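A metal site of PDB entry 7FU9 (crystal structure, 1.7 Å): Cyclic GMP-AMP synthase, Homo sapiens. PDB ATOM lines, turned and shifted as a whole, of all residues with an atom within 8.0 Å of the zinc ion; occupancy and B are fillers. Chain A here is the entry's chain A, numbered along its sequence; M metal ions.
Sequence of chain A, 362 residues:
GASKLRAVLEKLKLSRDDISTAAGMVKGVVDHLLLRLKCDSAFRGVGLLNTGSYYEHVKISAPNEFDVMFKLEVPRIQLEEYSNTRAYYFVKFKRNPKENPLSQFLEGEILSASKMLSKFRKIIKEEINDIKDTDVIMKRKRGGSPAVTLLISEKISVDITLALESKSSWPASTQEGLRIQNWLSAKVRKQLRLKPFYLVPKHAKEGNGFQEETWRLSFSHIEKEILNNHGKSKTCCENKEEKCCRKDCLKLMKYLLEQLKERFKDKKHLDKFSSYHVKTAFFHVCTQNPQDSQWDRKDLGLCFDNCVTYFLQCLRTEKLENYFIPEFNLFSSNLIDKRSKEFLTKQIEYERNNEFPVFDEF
The backbone carbonyl oxygen (O) of Cys 237 lies within hydrogen-bond range of the side-chain amino group (NZ) of Lys 243.
A ring nitrogen (ND1) of His 230 lies within hydrogen-bond range of the backbone carbonyl oxygen (O) of Leu 227.
O of Glu 242 is in hydrogen-bond range of N of Cys 237, at 2.5 Å.
NH2 of Arg 246 lies close to SG of Cys 236 (3.7 Å).
The guanidinium group (NE) of Arg 246 sits at hydrogen-bond distance from the backbone carbonyl oxygen (O) of His 230, 3.3 Å away.
The side-chain sulfur (SG) of Cys 244 lies close to the guanidinium group (NH2) of Arg 246 (3.4 Å).
The zinc ion is bound by NE2 of His 230 (2.1 Å), SG of Cys 237 (2.3 Å), SG of Cys 236 (2.3 Å) and SG of Cys 244 (2.4 Å).
The zinc ion has four donor atoms within binding distance.
Four residues have an atom within 4 Å of the zinc ion: His 230, Cys 236, Cys 237 and Cys 244.
The nearest printed residue that does not touch the zinc ion is Arg 246 (4.4 Å).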
ATOM      1  N   LEU A 227      13.698   7.934 -24.645  1.00  0.00           N
ATOM      2  CA  LEU A 227      14.571   8.954 -25.223  1.00  0.00           C
ATOM      3  C   LEU A 227      13.932  10.332 -25.155  1.00  0.00           C
ATOM      4  O   LEU A 227      14.607  11.337 -24.915  1.00  0.00           O
ATOM      5  CB  LEU A 227      14.857   8.614 -26.690  1.00  0.00           C
ATOM      6  CG  LEU A 227      16.042   7.697 -26.913  1.00  0.00           C
ATOM      7  CD1 LEU A 227      16.199   7.384 -28.410  1.00  0.00           C
ATOM      8  CD2 LEU A 227      17.257   8.404 -26.337  1.00  0.00           C
ATOM      9  N   ASN A 228      12.629  10.392 -25.393  1.00  0.00           N
ATOM     10  CA  ASN A 228      11.855  11.624 -25.405  1.00  0.00           C
ATOM     11  C   ASN A 228      11.269  12.015 -24.058  1.00  0.00           C
ATOM     12  O   ASN A 228      10.614  13.063 -23.957  1.00  0.00           O
ATOM     13  CB  ASN A 228      10.699  11.509 -26.407  1.00  0.00           C
ATOM     14  CG  ASN A 228      11.187  11.493 -27.839  1.00  0.00           C
ATOM     15  OD1 ASN A 228      12.237  12.057 -28.171  1.00  0.00           O
ATOM     16  ND2 ASN A 228      10.412  10.855 -28.711  1.00  0.00           N
ATOM     17  N   ASN A 229      11.440  11.181 -23.037  1.00  0.00           N
ATOM     18  CA  ASN A 229      10.958  11.447 -21.681  1.00  0.00           C
ATOM     19  C   ASN A 229      12.038  10.875 -20.766  1.00  0.00           C
ATOM     20  O   ASN A 229      11.892   9.849 -20.091  1.00  0.00           O
ATOM     21  CB  ASN A 229       9.565  10.864 -21.435  1.00  0.00           C
ATOM     22  CG  ASN A 229       8.936  11.362 -20.143  1.00  0.00           C
ATOM     23  OD1 ASN A 229       9.544  12.144 -19.396  1.00  0.00           O
ATOM     24  ND2 ASN A 229       7.722  10.920 -19.875  1.00  0.00           N
ATOM     25  N   HIS A 230      13.197  11.544 -20.771  1.00  0.00           N
ATOM     26  CA  HIS A 230      14.475  10.929 -20.425  1.00  0.00           C
ATOM     27  C   HIS A 230      15.062  11.412 -19.110  1.00  0.00           C
ATOM     28  O   HIS A 230      16.155  10.950 -18.729  1.00  0.00           O
ATOM     29  CB  HIS A 230      15.500  11.208 -21.526  1.00  0.00           C
ATOM     30  CG  HIS A 230      15.708  12.683 -21.770  1.00  0.00           C
ATOM     31  ND1 HIS A 230      15.422  13.286 -22.975  1.00  0.00           N
ATOM     32  CD2 HIS A 230      16.134  13.666 -20.940  1.00  0.00           C
ATOM     33  CE1 HIS A 230      15.673  14.588 -22.883  1.00  0.00           C
ATOM     34  NE2 HIS A 230      16.075  14.852 -21.641  1.00  0.00           N
ATOM     35  N   GLY A 231      14.454  12.368 -18.437  1.00  0.00           N
ATOM     36  CA  GLY A 231      15.042  12.884 -17.222  1.00  0.00           C
ATOM     37  C   GLY A 231      14.512  12.209 -15.985  1.00  0.00           C
ATOM     38  O   GLY A 231      13.469  11.577 -15.982  1.00  0.00           O
ATOM     39  N   LYS A 232      15.272  12.334 -14.900  1.00  0.00           N
ATOM     40  CA  LYS A 232      14.703  12.058 -13.589  1.00  0.00           C
ATOM     41  C   LYS A 232      13.616  13.088 -13.280  1.00  0.00           C
ATOM     42  O   LYS A 232      12.532  12.735 -12.800  1.00  0.00           O
ATOM     43  CB  LYS A 232      15.793  12.088 -12.522  1.00  0.00           C
ATOM     44  CG  LYS A 232      15.177  12.033 -11.098  1.00  0.00           C
ATOM     45  CD  LYS A 232      16.167  11.838  -9.952  1.00  0.00           C
ATOM     46  CE  LYS A 232      16.897  10.472 -10.018  1.00  0.00           C
ATOM     47  NZ  LYS A 232      15.983   9.281 -10.102  1.00  0.00           N
ATOM     48  N   SER A 233      13.893  14.357 -13.542  1.00  0.00           N
ATOM     49  CA  SER A 233      12.836  15.363 -13.478  1.00  0.00           C
ATOM     50  C   SER A 233      11.858  15.192 -14.633  1.00  0.00           C
ATOM     51  O   SER A 233      12.262  15.077 -15.793  1.00  0.00           O
ATOM     52  CB  SER A 233      13.431  16.759 -13.551  1.00  0.00           C
ATOM     53  OG  SER A 233      12.352  17.693 -13.563  1.00  0.00           O
ATOM     54  N   THR A 235      10.191  17.542 -15.850  1.00  0.00           N
ATOM     55  CA  THR A 235      10.359  18.703 -16.708  1.00  0.00           C
ATOM     56  C   THR A 235      11.786  18.848 -17.267  1.00  0.00           C
ATOM     57  O   THR A 235      12.145  19.942 -17.724  1.00  0.00           O
ATOM     58  CB  THR A 235       9.972  19.994 -15.975  1.00  0.00           C
ATOM     59  OG1 THR A 235      10.605  20.045 -14.667  1.00  0.00           O
ATOM     60  CG2 THR A 235       8.460  20.072 -15.787  1.00  0.00           C
ATOM     61  N   CYS A 236      12.607  17.779 -17.254  1.00  0.00           N
ATOM     62  CA  CYS A 236      13.907  17.806 -17.935  1.00  0.00           C
ATOM     63  C   CYS A 236      13.745  18.292 -19.375  1.00  0.00           C
ATOM     64  O   CYS A 236      12.874  17.813 -20.099  1.00  0.00           O
ATOM     65  CB  CYS A 236      14.553  16.410 -17.951  1.00  0.00           C
ATOM     66  SG  CYS A 236      16.344  16.412 -18.321  1.00  0.00           S
ATOM     67  N   CYS A 237      14.574  19.269 -19.780  1.00  0.00           N
ATOM     68  CA  CYS A 237      14.544  19.881 -21.115  1.00  0.00           C
ATOM     69  C   CYS A 237      13.209  20.608 -21.461  1.00  0.00           C
ATOM     70  O   CYS A 237      13.023  21.034 -22.614  1.00  0.00           O
ATOM     71  CB  CYS A 237      14.903  18.815 -22.178  1.00  0.00           C
ATOM     72  SG  CYS A 237      16.653  18.322 -22.046  1.00  0.00           S
ATOM     73  N   GLU A 238      12.310  20.860 -20.503  1.00  0.00           N
ATOM     74  CA  GLU A 238      11.141  21.686 -20.805  1.00  0.00           C
ATOM     75  C   GLU A 238      11.309  23.142 -20.412  1.00  0.00           C
ATOM     76  O   GLU A 238      10.403  23.956 -20.621  1.00  0.00           O
ATOM     77  CB  GLU A 238       9.882  21.125 -20.112  1.00  0.00           C
ATOM     78  CG  GLU A 238       9.431  19.771 -20.665  1.00  0.00           C
ATOM     79  CD  GLU A 238       8.027  19.374 -20.171  1.00  0.00           C
ATOM     80  OE1 GLU A 238       7.423  20.055 -19.305  1.00  0.00           O
ATOM     81  OE2 GLU A 238       7.510  18.356 -20.667  1.00  0.00           O
ATOM     82  N   GLU A 242      16.583  23.448 -16.900  1.00  0.00           N
ATOM     83  CA  GLU A 242      16.781  22.009 -16.865  1.00  0.00           C
ATOM     84  C   GLU A 242      17.152  21.512 -18.240  1.00  0.00           C
ATOM     85  O   GLU A 242      16.493  20.639 -18.816  1.00  0.00           O
ATOM     86  CB  GLU A 242      15.537  21.267 -16.368  1.00  0.00           C
ATOM     87  CG  GLU A 242      15.041  21.686 -14.955  1.00  0.00           C
ATOM     88  CD  GLU A 242      13.825  20.879 -14.550  1.00  0.00           C
ATOM     89  OE1 GLU A 242      13.967  19.635 -14.381  1.00  0.00           O
ATOM     90  OE2 GLU A 242      12.723  21.473 -14.444  1.00  0.00           O
ATOM     91  N   LYS A 243      18.264  22.006 -18.771  1.00  0.00           N
ATOM     92  CA  LYS A 243      18.752  21.575 -20.077  1.00  0.00           C
ATOM     93  C   LYS A 243      19.864  20.542 -19.882  1.00  0.00           C
ATOM     94  O   LYS A 243      20.959  20.880 -19.430  1.00  0.00           O
ATOM     95  CB  LYS A 243      19.263  22.783 -20.858  1.00  0.00           C
ATOM     96  CG  LYS A 243      18.124  23.662 -21.448  1.00  0.00           C
ATOM     97  CD  LYS A 243      17.088  22.750 -22.098  1.00  0.00           C
ATOM     98  CE  LYS A 243      16.348  23.340 -23.296  1.00  0.00           C
ATOM     99  NZ  LYS A 243      15.682  22.227 -24.071  1.00  0.00           N
ATOM    100  N   CYS A 244      19.595  19.287 -20.247  1.00  0.00           N
ATOM    101  CA  CYS A 244      20.609  18.237 -20.138  1.00  0.00           C
ATOM    102  C   CYS A 244      21.173  17.887 -21.519  1.00  0.00           C
ATOM    103  O   CYS A 244      20.630  18.297 -22.554  1.00  0.00           O
ATOM    104  CB  CYS A 244      20.065  16.966 -19.468  1.00  0.00           C
ATOM    105  SG  CYS A 244      19.059  15.801 -20.506  1.00  0.00           S
ATOM    106  N   CYS A 245      22.237  17.093 -21.537  1.00  0.00           N
ATOM    107  CA  CYS A 245      22.892  16.720 -22.795  1.00  0.00           C
ATOM    108  C   CYS A 245      22.730  15.234 -23.143  1.00  0.00           C
ATOM    109  O   CYS A 245      23.526  14.695 -23.925  1.00  0.00           O
ATOM    110  CB  CYS A 245      24.380  17.094 -22.763  1.00  0.00           C
ATOM    111  SG  CYS A 245      25.358  16.281 -21.477  1.00  0.00           S
ATOM    112  N   ARG A 246      21.698  14.569 -22.621  1.00  0.00           N
ATOM    113  CA  ARG A 246      21.544  13.128 -22.887  1.00  0.00           C
ATOM    114  C   ARG A 246      21.361  12.863 -24.380  1.00  0.00           C
ATOM    115  O   ARG A 246      22.028  11.981 -24.952  1.00  0.00           O
ATOM    116  CB  ARG A 246      20.373  12.565 -22.050  1.00  0.00           C
ATOM    117  CG  ARG A 246      20.643  12.324 -20.538  1.00  0.00           C
ATOM    118  CD  ARG A 246      19.390  11.655 -19.964  1.00  0.00           C
ATOM    119  NE  ARG A 246      19.406  11.375 -18.520  1.00  0.00           N
ATOM    120  CZ  ARG A 246      19.046  12.277 -17.605  1.00  0.00           C
ATOM    121  NH1 ARG A 246      19.033  11.933 -16.318  1.00  0.00           N
ATOM    122  NH2 ARG A 246      18.682  13.510 -17.980  1.00  0.00           N
ATOM    123  N   LYS A 247      20.442  13.572 -25.037  1.00  0.00           N
ATOM    124  CA  LYS A 247      20.230  13.322 -26.464  1.00  0.00           C
ATOM    125  C   LYS A 247      21.475  13.649 -27.273  1.00  0.00           C
ATOM    126  O   LYS A 247      21.809  12.951 -28.249  1.00  0.00           O
ATOM    127  CB  LYS A 247      19.027  14.108 -27.004  1.00  0.00           C
ATOM    128  CG  LYS A 247      17.659  13.494 -26.695  1.00  0.00           C
ATOM    129  CD  LYS A 247      16.556  14.238 -27.477  1.00  0.00           C
ATOM    130  CE  LYS A 247      15.166  13.795 -27.036  1.00  0.00           C
ATOM    131  NZ  LYS A 247      14.098  14.568 -27.734  1.00  0.00           N
ATOM    132  N   ASP A 292      19.818  14.077 -13.161  1.00  0.00           N
ATOM    133  CA  ASP A 292      19.927  15.063 -14.237  1.00  0.00           C
ATOM    134  C   ASP A 292      21.173  15.913 -14.069  1.00  0.00           C
ATOM    135  O   ASP A 292      21.741  16.385 -15.055  1.00  0.00           O
ATOM    136  CB  ASP A 292      18.676  15.947 -14.296  1.00  0.00           C
ATOM    137  CG  ASP A 292      17.408  15.171 -14.679  1.00  0.00           C
ATOM    138  OD1 ASP A 292      17.495  14.101 -15.347  1.00  0.00           O
ATOM    139  OD2 ASP A 292      16.305  15.658 -14.289  1.00  0.00           O
ATOM    140  N   TRP A 295      24.174  15.120 -16.155  1.00  0.00           N
ATOM    141  CA  TRP A 295      24.012  15.335 -17.586  1.00  0.00           C
ATOM    142  C   TRP A 295      23.788  16.803 -17.905  1.00  0.00           C
ATOM    143  O   TRP A 295      23.140  17.139 -18.894  1.00  0.00           O
ATOM    144  CB  TRP A 295      22.829  14.499 -18.109  1.00  0.00           C
ATOM    145  CG  TRP A 295      23.002  13.031 -17.967  1.00  0.00           C
ATOM    146  CD1 TRP A 295      22.575  12.239 -16.914  1.00  0.00           C
ATOM    147  CD2 TRP A 295      23.636  12.146 -18.899  1.00  0.00           C
ATOM    148  NE1 TRP A 295      22.904  10.925 -17.145  1.00  0.00           N
ATOM    149  CE2 TRP A 295      23.546  10.829 -18.356  1.00  0.00           C
ATOM    150  CE3 TRP A 295      24.262  12.326 -20.145  1.00  0.00           C
ATOM    151  CZ2 TRP A 295      24.085   9.712 -19.002  1.00  0.00           C
ATOM    152  CZ3 TRP A 295      24.791  11.186 -20.793  1.00  0.00           C
ATOM    153  CH2 TRP A 295      24.686   9.906 -20.226  1.00  0.00           C
HETATM  154 ZN    ZN M   1      16.794  16.517 -20.597  1.00  0.00          ZN
